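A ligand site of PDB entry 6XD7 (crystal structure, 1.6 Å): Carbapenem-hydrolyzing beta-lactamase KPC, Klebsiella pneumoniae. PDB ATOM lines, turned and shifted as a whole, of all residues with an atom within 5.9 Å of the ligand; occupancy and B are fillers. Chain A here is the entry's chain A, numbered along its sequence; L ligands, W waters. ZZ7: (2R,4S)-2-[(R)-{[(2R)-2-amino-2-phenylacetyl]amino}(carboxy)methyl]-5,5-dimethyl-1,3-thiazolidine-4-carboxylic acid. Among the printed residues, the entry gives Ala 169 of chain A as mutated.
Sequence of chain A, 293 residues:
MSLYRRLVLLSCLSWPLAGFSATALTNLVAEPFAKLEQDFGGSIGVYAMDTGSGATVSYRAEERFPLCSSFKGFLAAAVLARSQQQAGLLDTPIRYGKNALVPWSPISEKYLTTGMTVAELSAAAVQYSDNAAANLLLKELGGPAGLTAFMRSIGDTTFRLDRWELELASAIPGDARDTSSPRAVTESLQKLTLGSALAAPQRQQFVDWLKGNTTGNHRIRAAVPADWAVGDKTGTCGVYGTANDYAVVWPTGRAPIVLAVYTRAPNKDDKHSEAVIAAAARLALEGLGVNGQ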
ATOM      1  N   LEU A  67     -21.331  -4.761 -20.197  1.00  0.00           N
ATOM      2  CA  LEU A  67     -19.971  -4.481 -19.741  1.00  0.00           C
ATOM      3  C   LEU A  67     -19.907  -3.248 -18.860  1.00  0.00           C
ATOM      4  O   LEU A  67     -19.106  -3.182 -17.928  1.00  0.00           O
ATOM      5  CB  LEU A  67     -19.046  -4.306 -20.945  1.00  0.00           C
ATOM      6  CG  LEU A  67     -18.708  -5.569 -21.737  1.00  0.00           C
ATOM      7  CD1 LEU A  67     -18.273  -5.189 -23.157  1.00  0.00           C
ATOM      8  CD2 LEU A  67     -17.640  -6.388 -21.011  1.00  0.00           C
ATOM      9  N   CYS A  68     -20.697  -2.228 -19.180  1.00  0.00           N
ATOM     10  CA  CYS A  68     -20.595  -0.933 -18.508  1.00  0.00           C
ATOM     11  C   CYS A  68     -19.147  -0.464 -18.601  1.00  0.00           C
ATOM     12  O   CYS A  68     -18.432  -0.812 -19.555  1.00  0.00           O
ATOM     13  CB  CYS A  68     -21.128  -1.035 -17.077  1.00  0.00           C
ATOM     14  SG  CYS A  68     -22.757  -1.829 -16.955  1.00  0.00           S
ATOM     15  N   SER A  69     -18.672   0.277 -17.615  1.00  0.00           N
ATOM     16  CA  SER A  69     -17.295   0.748 -17.653  1.00  0.00           C
ATOM     17  C   SER A  69     -16.253  -0.358 -17.564  1.00  0.00           C
ATOM     18  O   SER A  69     -15.074  -0.049 -17.690  1.00  0.00           O
ATOM     19  CB  SER A  69     -17.047   1.756 -16.523  1.00  0.00           C
ATOM     20  OG  SER A  69     -17.589   3.017 -16.843  1.00  0.00           O
ATOM     21  N   SER A  70     -16.620  -1.619 -17.346  1.00  0.00           N
ATOM     22  CA  SER A  70     -15.561  -2.628 -17.219  1.00  0.00           C
ATOM     23  C   SER A  70     -14.841  -2.874 -18.538  1.00  0.00           C
ATOM     24  O   SER A  70     -13.738  -3.427 -18.522  1.00  0.00           O
ATOM     25  CB  SER A  70     -16.116  -3.930 -16.634  1.00  0.00           C
ATOM     26  OG  SER A  70     -16.878  -4.690 -17.574  1.00  0.00           O
ATOM     27  N   PHE A  71     -15.387  -2.431 -19.681  1.00  0.00           N
ATOM     28  CA  PHE A  71     -14.630  -2.517 -20.926  1.00  0.00           C
ATOM     29  C   PHE A  71     -13.321  -1.736 -20.860  1.00  0.00           C
ATOM     30  O   PHE A  71     -12.397  -2.034 -21.627  1.00  0.00           O
ATOM     31  CB  PHE A  71     -15.464  -2.038 -22.116  1.00  0.00           C
ATOM     32  CG  PHE A  71     -15.423  -0.535 -22.344  1.00  0.00           C
ATOM     33  CD1 PHE A  71     -16.309   0.309 -21.694  1.00  0.00           C
ATOM     34  CD2 PHE A  71     -14.497   0.010 -23.238  1.00  0.00           C
ATOM     35  CE1 PHE A  71     -16.253   1.692 -21.920  1.00  0.00           C
ATOM     36  CE2 PHE A  71     -14.430   1.384 -23.454  1.00  0.00           C
ATOM     37  CZ  PHE A  71     -15.314   2.223 -22.791  1.00  0.00           C
ATOM     38  N   LYS A  72     -13.224  -0.740 -19.967  1.00  0.00           N
ATOM     39  CA  LYS A  72     -12.048   0.126 -19.978  1.00  0.00           C
ATOM     40  C   LYS A  72     -10.786  -0.636 -19.566  1.00  0.00           C
ATOM     41  O   LYS A  72      -9.695  -0.246 -19.967  1.00  0.00           O
ATOM     42  CB  LYS A  72     -12.283   1.325 -19.062  1.00  0.00           C
ATOM     43  CG  LYS A  72     -13.386   2.258 -19.577  1.00  0.00           C
ATOM     44  CD  LYS A  72     -13.826   3.237 -18.498  1.00  0.00           C
ATOM     45  CE  LYS A  72     -14.949   4.146 -19.003  1.00  0.00           C
ATOM     46  NZ  LYS A  72     -15.760   4.770 -17.890  1.00  0.00           N
ATOM     47  N   PRO A 103     -19.501  13.658 -19.107  1.00  0.00           N
ATOM     48  CA  PRO A 103     -19.709  13.600 -17.658  1.00  0.00           C
ATOM     49  C   PRO A 103     -18.893  12.482 -17.018  1.00  0.00           C
ATOM     50  O   PRO A 103     -18.645  11.444 -17.635  1.00  0.00           O
ATOM     51  CB  PRO A 103     -21.210  13.371 -17.516  1.00  0.00           C
ATOM     52  CG  PRO A 103     -21.794  13.903 -18.770  1.00  0.00           C
ATOM     53  CD  PRO A 103     -20.777  13.724 -19.852  1.00  0.00           C
ATOM     54  N   TRP A 104     -18.471  12.723 -15.775  1.00  0.00           N
ATOM     55  CA  TRP A 104     -17.689  11.768 -14.982  1.00  0.00           C
ATOM     56  C   TRP A 104     -16.356  11.452 -15.658  1.00  0.00           C
ATOM     57  O   TRP A 104     -16.016  10.327 -16.011  1.00  0.00           O
ATOM     58  CB  TRP A 104     -18.526  10.523 -14.655  1.00  0.00           C
ATOM     59  CG  TRP A 104     -19.774  10.978 -13.963  1.00  0.00           C
ATOM     60  CD1 TRP A 104     -19.853  11.582 -12.720  1.00  0.00           C
ATOM     61  CD2 TRP A 104     -21.114  10.956 -14.473  1.00  0.00           C
ATOM     62  NE1 TRP A 104     -21.161  11.890 -12.428  1.00  0.00           N
ATOM     63  CE2 TRP A 104     -21.950  11.523 -13.495  1.00  0.00           C
ATOM     64  CE3 TRP A 104     -21.681  10.490 -15.661  1.00  0.00           C
ATOM     65  CZ2 TRP A 104     -23.330  11.641 -13.665  1.00  0.00           C
ATOM     66  CZ3 TRP A 104     -23.048  10.606 -15.826  1.00  0.00           C
ATOM     67  CH2 TRP A 104     -23.855  11.180 -14.843  1.00  0.00           C
ATOM     68  N   TYR A 128      -9.863   5.300 -12.569  1.00  0.00           N
ATOM     69  CA  TYR A 128     -10.905   6.245 -12.210  1.00  0.00           C
ATOM     70  C   TYR A 128     -12.117   6.151 -13.128  1.00  0.00           C
ATOM     71  O   TYR A 128     -13.059   6.926 -12.985  1.00  0.00           O
ATOM     72  CB  TYR A 128     -10.363   7.677 -12.208  1.00  0.00           C
ATOM     73  CG  TYR A 128      -9.364   7.919 -11.120  1.00  0.00           C
ATOM     74  CD1 TYR A 128      -9.782   8.324  -9.862  1.00  0.00           C
ATOM     75  CD2 TYR A 128      -8.012   7.721 -11.322  1.00  0.00           C
ATOM     76  CE1 TYR A 128      -8.865   8.535  -8.848  1.00  0.00           C
ATOM     77  CE2 TYR A 128      -7.098   7.937 -10.320  1.00  0.00           C
ATOM     78  CZ  TYR A 128      -7.529   8.341  -9.091  1.00  0.00           C
ATOM     79  OH  TYR A 128      -6.625   8.552  -8.082  1.00  0.00           O
ATOM     80  N   SER A 129     -12.077   5.188 -14.044  1.00  0.00           N
ATOM     81  CA  SER A 129     -13.150   4.967 -15.021  1.00  0.00           C
ATOM     82  C   SER A 129     -13.477   6.280 -15.740  1.00  0.00           C
ATOM     83  O   SER A 129     -14.636   6.575 -16.016  1.00  0.00           O
ATOM     84  CB  SER A 129     -14.384   4.350 -14.356  1.00  0.00           C
ATOM     85  OG  SER A 129     -15.241   3.771 -15.310  1.00  0.00           O
ATOM     86  N   ASP A 130     -12.441   7.046 -16.058  1.00  0.00           N
ATOM     87  CA  ASP A 130     -12.568   8.346 -16.709  1.00  0.00           C
ATOM     88  C   ASP A 130     -13.194   8.204 -18.101  1.00  0.00           C
ATOM     89  O   ASP A 130     -12.632   7.542 -18.973  1.00  0.00           O
ATOM     90  CB  ASP A 130     -11.189   8.995 -16.807  1.00  0.00           C
ATOM     91  CG  ASP A 130     -11.245  10.458 -17.194  1.00  0.00           C
ATOM     92  OD1 ASP A 130     -11.602  10.740 -18.350  1.00  0.00           O
ATOM     93  OD2 ASP A 130     -10.910  11.323 -16.345  1.00  0.00           O
ATOM     94  N   ASN A 131     -14.377   8.796 -18.295  1.00  0.00           N
ATOM     95  CA  ASN A 131     -15.107   8.553 -19.535  1.00  0.00           C
ATOM     96  C   ASN A 131     -14.452   9.237 -20.727  1.00  0.00           C
ATOM     97  O   ASN A 131     -14.379   8.661 -21.817  1.00  0.00           O
ATOM     98  CB  ASN A 131     -16.557   9.028 -19.408  1.00  0.00           C
ATOM     99  CG  ASN A 131     -17.417   8.034 -18.660  1.00  0.00           C
ATOM    100  OD1 ASN A 131     -17.316   6.821 -18.858  1.00  0.00           O
ATOM    101  ND2 ASN A 131     -18.286   8.548 -17.814  1.00  0.00           N
ATOM    102  N   GLU A 165     -18.855   5.914 -24.735  1.00  0.00           N
ATOM    103  CA  GLU A 165     -19.419   6.535 -23.536  1.00  0.00           C
ATOM    104  C   GLU A 165     -20.136   7.811 -23.952  1.00  0.00           C
ATOM    105  O   GLU A 165     -19.643   8.568 -24.790  1.00  0.00           O
ATOM    106  CB  GLU A 165     -18.323   6.828 -22.503  1.00  0.00           C
ATOM    107  CG  GLU A 165     -17.716   5.545 -21.917  1.00  0.00           C
ATOM    108  CD  GLU A 165     -18.581   4.906 -20.825  1.00  0.00           C
ATOM    109  OE1 GLU A 165     -19.808   5.175 -20.777  1.00  0.00           O
ATOM    110  OE2 GLU A 165     -18.058   4.058 -20.064  1.00  0.00           O
ATOM    111  N   LEU A 166     -21.345   8.041 -23.417  1.00  0.00           N
ATOM    112  CA  LEU A 166     -21.980   7.276 -22.341  1.00  0.00           C
ATOM    113  C   LEU A 166     -23.086   6.361 -22.873  1.00  0.00           C
ATOM    114  O   LEU A 166     -23.782   5.687 -22.106  1.00  0.00           O
ATOM    115  CB  LEU A 166     -22.602   8.244 -21.345  1.00  0.00           C
ATOM    116  CG  LEU A 166     -21.684   9.077 -20.455  1.00  0.00           C
ATOM    117  CD1 LEU A 166     -22.518  10.154 -19.781  1.00  0.00           C
ATOM    118  CD2 LEU A 166     -21.026   8.195 -19.417  1.00  0.00           C
ATOM    119  N   LEU A 168     -23.063   3.608 -24.365  1.00  0.00           N
ATOM    120  CA  LEU A 168     -22.946   2.160 -24.219  1.00  0.00           C
ATOM    121  C   LEU A 168     -23.543   1.650 -22.921  1.00  0.00           C
ATOM    122  O   LEU A 168     -23.660   0.429 -22.747  1.00  0.00           O
ATOM    123  CB  LEU A 168     -21.480   1.719 -24.320  1.00  0.00           C
ATOM    124  CG  LEU A 168     -20.476   2.275 -23.298  1.00  0.00           C
ATOM    125  CD1 LEU A 168     -20.469   1.466 -22.027  1.00  0.00           C
ATOM    126  CD2 LEU A 168     -19.062   2.308 -23.877  1.00  0.00           C
ATOM    127  N   ALA A 169     -23.887   2.535 -21.987  1.00  0.00           N
ATOM    128  CA  ALA A 169     -24.305   2.117 -20.650  1.00  0.00           C
ATOM    129  C   ALA A 169     -25.824   1.990 -20.501  1.00  0.00           C
ATOM    130  O   ALA A 169     -26.327   2.041 -19.373  1.00  0.00           O
ATOM    131  CB  ALA A 169     -23.765   3.094 -19.611  1.00  0.00           C
ATOM    132  N   LYS A 233     -11.204  -4.097 -12.093  1.00  0.00           N
ATOM    133  CA  LYS A 233     -11.855  -3.054 -12.878  1.00  0.00           C
ATOM    134  C   LYS A 233     -13.350  -3.203 -12.672  1.00  0.00           C
ATOM    135  O   LYS A 233     -13.886  -4.300 -12.849  1.00  0.00           O
ATOM    136  CB  LYS A 233     -11.517  -3.157 -14.367  1.00  0.00           C
ATOM    137  CG  LYS A 233     -12.180  -2.078 -15.221  1.00  0.00           C
ATOM    138  CD  LYS A 233     -11.524  -0.703 -14.994  1.00  0.00           C
ATOM    139  CE  LYS A 233     -12.403   0.430 -15.489  1.00  0.00           C
ATOM    140  NZ  LYS A 233     -13.488   0.835 -14.518  1.00  0.00           N
ATOM    141  N   THR A 234     -14.023  -2.105 -12.290  1.00  0.00           N
ATOM    142  CA  THR A 234     -15.457  -2.091 -12.015  1.00  0.00           C
ATOM    143  C   THR A 234     -16.234  -1.545 -13.205  1.00  0.00           C
ATOM    144  O   THR A 234     -15.693  -0.871 -14.088  1.00  0.00           O
ATOM    145  CB  THR A 234     -15.767  -1.240 -10.790  1.00  0.00           C
ATOM    146  OG1 THR A 234     -15.501   0.146 -11.084  1.00  0.00           O
ATOM    147  CG2 THR A 234     -14.897  -1.661  -9.607  1.00  0.00           C
ATOM    148  N   GLY A 235     -17.540  -1.834 -13.209  1.00  0.00           N
ATOM    149  CA  GLY A 235     -18.437  -1.198 -14.164  1.00  0.00           C
ATOM    150  C   GLY A 235     -19.762  -0.886 -13.492  1.00  0.00           C
ATOM    151  O   GLY A 235     -20.221  -1.673 -12.650  1.00  0.00           O
ATOM    152  N   THR A 236     -20.383   0.248 -13.824  1.00  0.00           N
ATOM    153  CA  THR A 236     -21.650   0.624 -13.200  1.00  0.00           C
ATOM    154  C   THR A 236     -22.512   1.332 -14.242  1.00  0.00           C
ATOM    155  O   THR A 236     -22.388   2.539 -14.439  1.00  0.00           O
ATOM    156  CB  THR A 236     -21.432   1.514 -11.979  1.00  0.00           C
ATOM    157  OG1 THR A 236     -20.481   0.882 -11.096  1.00  0.00           O
ATOM    158  CG2 THR A 236     -22.746   1.713 -11.232  1.00  0.00           C
ATOM    159  N   CYS A 237     -23.396   0.580 -14.888  1.00  0.00           N
ATOM    160  CA  CYS A 237     -24.422   1.205 -15.711  1.00  0.00           C
ATOM    161  C   CYS A 237     -25.465   1.889 -14.851  1.00  0.00           C
ATOM    162  O   CYS A 237     -26.083   2.871 -15.286  1.00  0.00           O
ATOM    163  CB  CYS A 237     -25.107   0.161 -16.622  1.00  0.00           C
ATOM    164  SG  CYS A 237     -24.050  -0.522 -17.960  1.00  0.00           S
ATOM    165  N   GLY A 238     -25.683   1.392 -13.629  1.00  0.00           N
ATOM    166  CA  GLY A 238     -26.655   1.957 -12.717  1.00  0.00           C
ATOM    167  C   GLY A 238     -28.094   1.566 -13.006  1.00  0.00           C
ATOM    168  O   GLY A 238     -28.774   0.979 -12.159  1.00  0.00           O
ATOM    169  N   VAL A 239     -28.564   1.906 -14.216  1.00  0.00           N
ATOM    170  CA  VAL A 239     -29.913   1.528 -14.590  1.00  0.00           C
ATOM    171  C   VAL A 239     -29.997   0.001 -14.636  1.00  0.00           C
ATOM    172  O   VAL A 239     -28.992  -0.709 -14.757  1.00  0.00           O
ATOM    173  CB  VAL A 239     -30.299   2.124 -15.954  1.00  0.00           C
ATOM    174  CG1 VAL A 239     -30.538   3.618 -15.820  1.00  0.00           C
ATOM    175  CG2 VAL A 239     -29.213   1.834 -16.971  1.00  0.00           C
ATOM    176  N   HIS A 272     -28.495  -0.955  -8.354  1.00  0.00           N
ATOM    177  CA  HIS A 272     -27.403  -1.914  -8.293  1.00  0.00           C
ATOM    178  C   HIS A 272     -26.942  -2.037  -6.843  1.00  0.00           C
ATOM    179  O   HIS A 272     -27.269  -1.200  -6.011  1.00  0.00           O
ATOM    180  CB  HIS A 272     -26.256  -1.506  -9.206  1.00  0.00           C
ATOM    181  CG  HIS A 272     -25.445  -0.372  -8.667  1.00  0.00           C
ATOM    182  ND1 HIS A 272     -25.859   0.936  -8.737  1.00  0.00           N
ATOM    183  CD2 HIS A 272     -24.239  -0.350  -8.051  1.00  0.00           C
ATOM    184  CE1 HIS A 272     -24.950   1.716  -8.179  1.00  0.00           C
ATOM    185  NE2 HIS A 272     -23.954   0.959  -7.756  1.00  0.00           N
HETATM  186  O1  ZZ7 L   1     -18.602   4.545 -12.056  1.00  0.00           O
HETATM  187  C2  ZZ7 L   1     -18.770   4.104 -13.225  1.00  0.00           C
HETATM  188  O2  ZZ7 L   1     -18.148   3.095 -13.661  1.00  0.00           O
HETATM  189  C12 ZZ7 L   1     -19.715   4.721 -14.132  1.00  0.00           C
HETATM  190  C6  ZZ7 L   1     -19.297   6.308 -14.437  1.00  0.00           C
HETATM  191  C1  ZZ7 L   1     -17.812   6.450 -14.744  1.00  0.00           C
HETATM  192  C16 ZZ7 L   1     -19.674   7.215 -13.268  1.00  0.00           C
HETATM  193  S1  ZZ7 L   1     -20.338   6.704 -15.914  1.00  0.00           S
HETATM  194  N3  ZZ7 L   1     -19.556   4.020 -15.410  1.00  0.00           N
HETATM  195  C13 ZZ7 L   1     -19.951   5.106 -16.739  1.00  0.00           C
HETATM  196  C14 ZZ7 L   1     -21.183   4.482 -17.459  1.00  0.00           C
HETATM  197  C15 ZZ7 L   1     -20.747   3.070 -17.757  1.00  0.00           C
HETATM  198  O4  ZZ7 L   1     -21.039   2.138 -16.973  1.00  0.00           O
HETATM  199  N1  ZZ7 L   1     -22.326   4.535 -16.559  1.00  0.00           N
HETATM  200  C3  ZZ7 L   1     -23.277   5.467 -16.709  1.00  0.00           C
HETATM  201  O3  ZZ7 L   1     -23.257   6.308 -17.613  1.00  0.00           O
HETATM  202  C4  ZZ7 L   1     -24.425   5.440 -15.700  1.00  0.00           C
HETATM  203  N2  ZZ7 L   1     -25.540   6.189 -16.257  1.00  0.00           N
HETATM  204  C5  ZZ7 L   1     -23.978   6.036 -14.354  1.00  0.00           C
HETATM  205  C7  ZZ7 L   1     -23.646   7.376 -14.236  1.00  0.00           C
HETATM  206  C8  ZZ7 L   1     -23.234   7.872 -13.002  1.00  0.00           C
HETATM  207  C9  ZZ7 L   1     -23.166   7.039 -11.895  1.00  0.00           C
HETATM  208  C10 ZZ7 L   1     -23.489   5.695 -12.017  1.00  0.00           C
HETATM  209  C11 ZZ7 L   1     -23.896   5.202 -13.243  1.00  0.00           C
HETATM  210  OXT ZZ7 L   1     -20.065   2.841 -18.787  1.00  0.00           O
HETATM  211  O   HOH W   1     -17.785   1.741 -11.413  1.00  0.00           O
HETATM  212  O   HOH W   2     -19.830   8.683 -10.627  1.00  0.00           O
HETATM  213  O   HOH W   3     -26.875   4.438 -18.384  1.00  0.00           O
HETATM  214  O   HOH W   4     -15.436   8.538 -13.475  1.00  0.00           O
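The backbone NH of Ser 69 is in hydrogen-bond range of an oxygen (O4) of the ligand, 3.1 Å away.
The side-chain hydroxyl (OG) of Ser 69 is in hydrogen-bond range of a nitrogen (N3) of the ligand, at 2.6 Å.
The side-chain carboxylate of Glu 165 sits close to an oxygen (OXT) of the ligand.
The backbone carbonyl oxygen (O) of Thr 236 sits at hydrogen-bond distance from a nitrogen (N1) of the ligand, 2.9 Å away.
N2 of the ligand sits close to O of Cys 237, at 3.5 Å.
A sulfur (S1) of the ligand sits close to the side-chain amide nitrogen (ND2) of Asn 131, at 3.3 Å.
The side-chain hydroxyl (OG) of Ser 129 sits at hydrogen-bond distance from an oxygen (O2) of the ligand (3.4 Å).
OE2 of Glu 165 sits at hydrogen-bond distance from OG of Ser 69, at 3.4 Å.
The side-chain hydroxyl (OG) of Ser 69 sits at hydrogen-bond distance from the side-chain hydroxyl (OG) of Ser 129, 2.9 Å away.
The side-chain amino group (NZ) of Lys 72 sits at hydrogen-bond distance from the side-chain hydroxyl (OG) of Ser 69, 2.7 Å away.
OE2 of Glu 165 lies within salt-bridge range of NZ of Lys 72 (3.2 Å).
The side-chain sulfur (SG) of Cys 237 is disulfide-bonded to the side-chain sulfur (SG) of Cys 68 (2.1 Å).
NZ of Lys 72 is in hydrogen-bond range of OD1 of Asn 131 (2.8 Å).
ND2 of Asn 131 is in hydrogen-bond range of O of Pro 103 (2.9 Å).
OG of Ser 129 sits at hydrogen-bond distance from NZ of Lys 72, 2.8 Å away.
Cys 68 touches the ligand.
Trp 104 touches the ligand (CZ3 to C7, 3.6 Å).
CD2 of Leu 166 touches O3 of the ligand, at 3.4 Å.
Leu 168 touches the ligand (CD1 to OXT, 3.5 Å).
CB of Ala 169 touches C15 of the ligand (3.5 Å).
Hydrophobic or aromatic side chains that line the ligand: Trp 104, Leu 166, Leu 168 and Ala 169.
Within 4 Å of the ligand: Cys 68, Ser 69, Trp 104, Ser 129, Asn 131, Glu 165, Leu 166, Leu 168, Ala 169, Thr 236 and Cys 237.
The nearest printed residue that does not touch the ligand is Lys 72 (4.1 Å).
Water W1 lies within hydrogen-bond range of O2 of the ligand, OG1 of Thr 234 and OG1 of Thr 236.
Water W3 lies within hydrogen-bond range of the backbone carbonyl oxygen of Ala 169 (2.7 Å) and a nitrogen (N2) of the ligand (3.1 Å).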
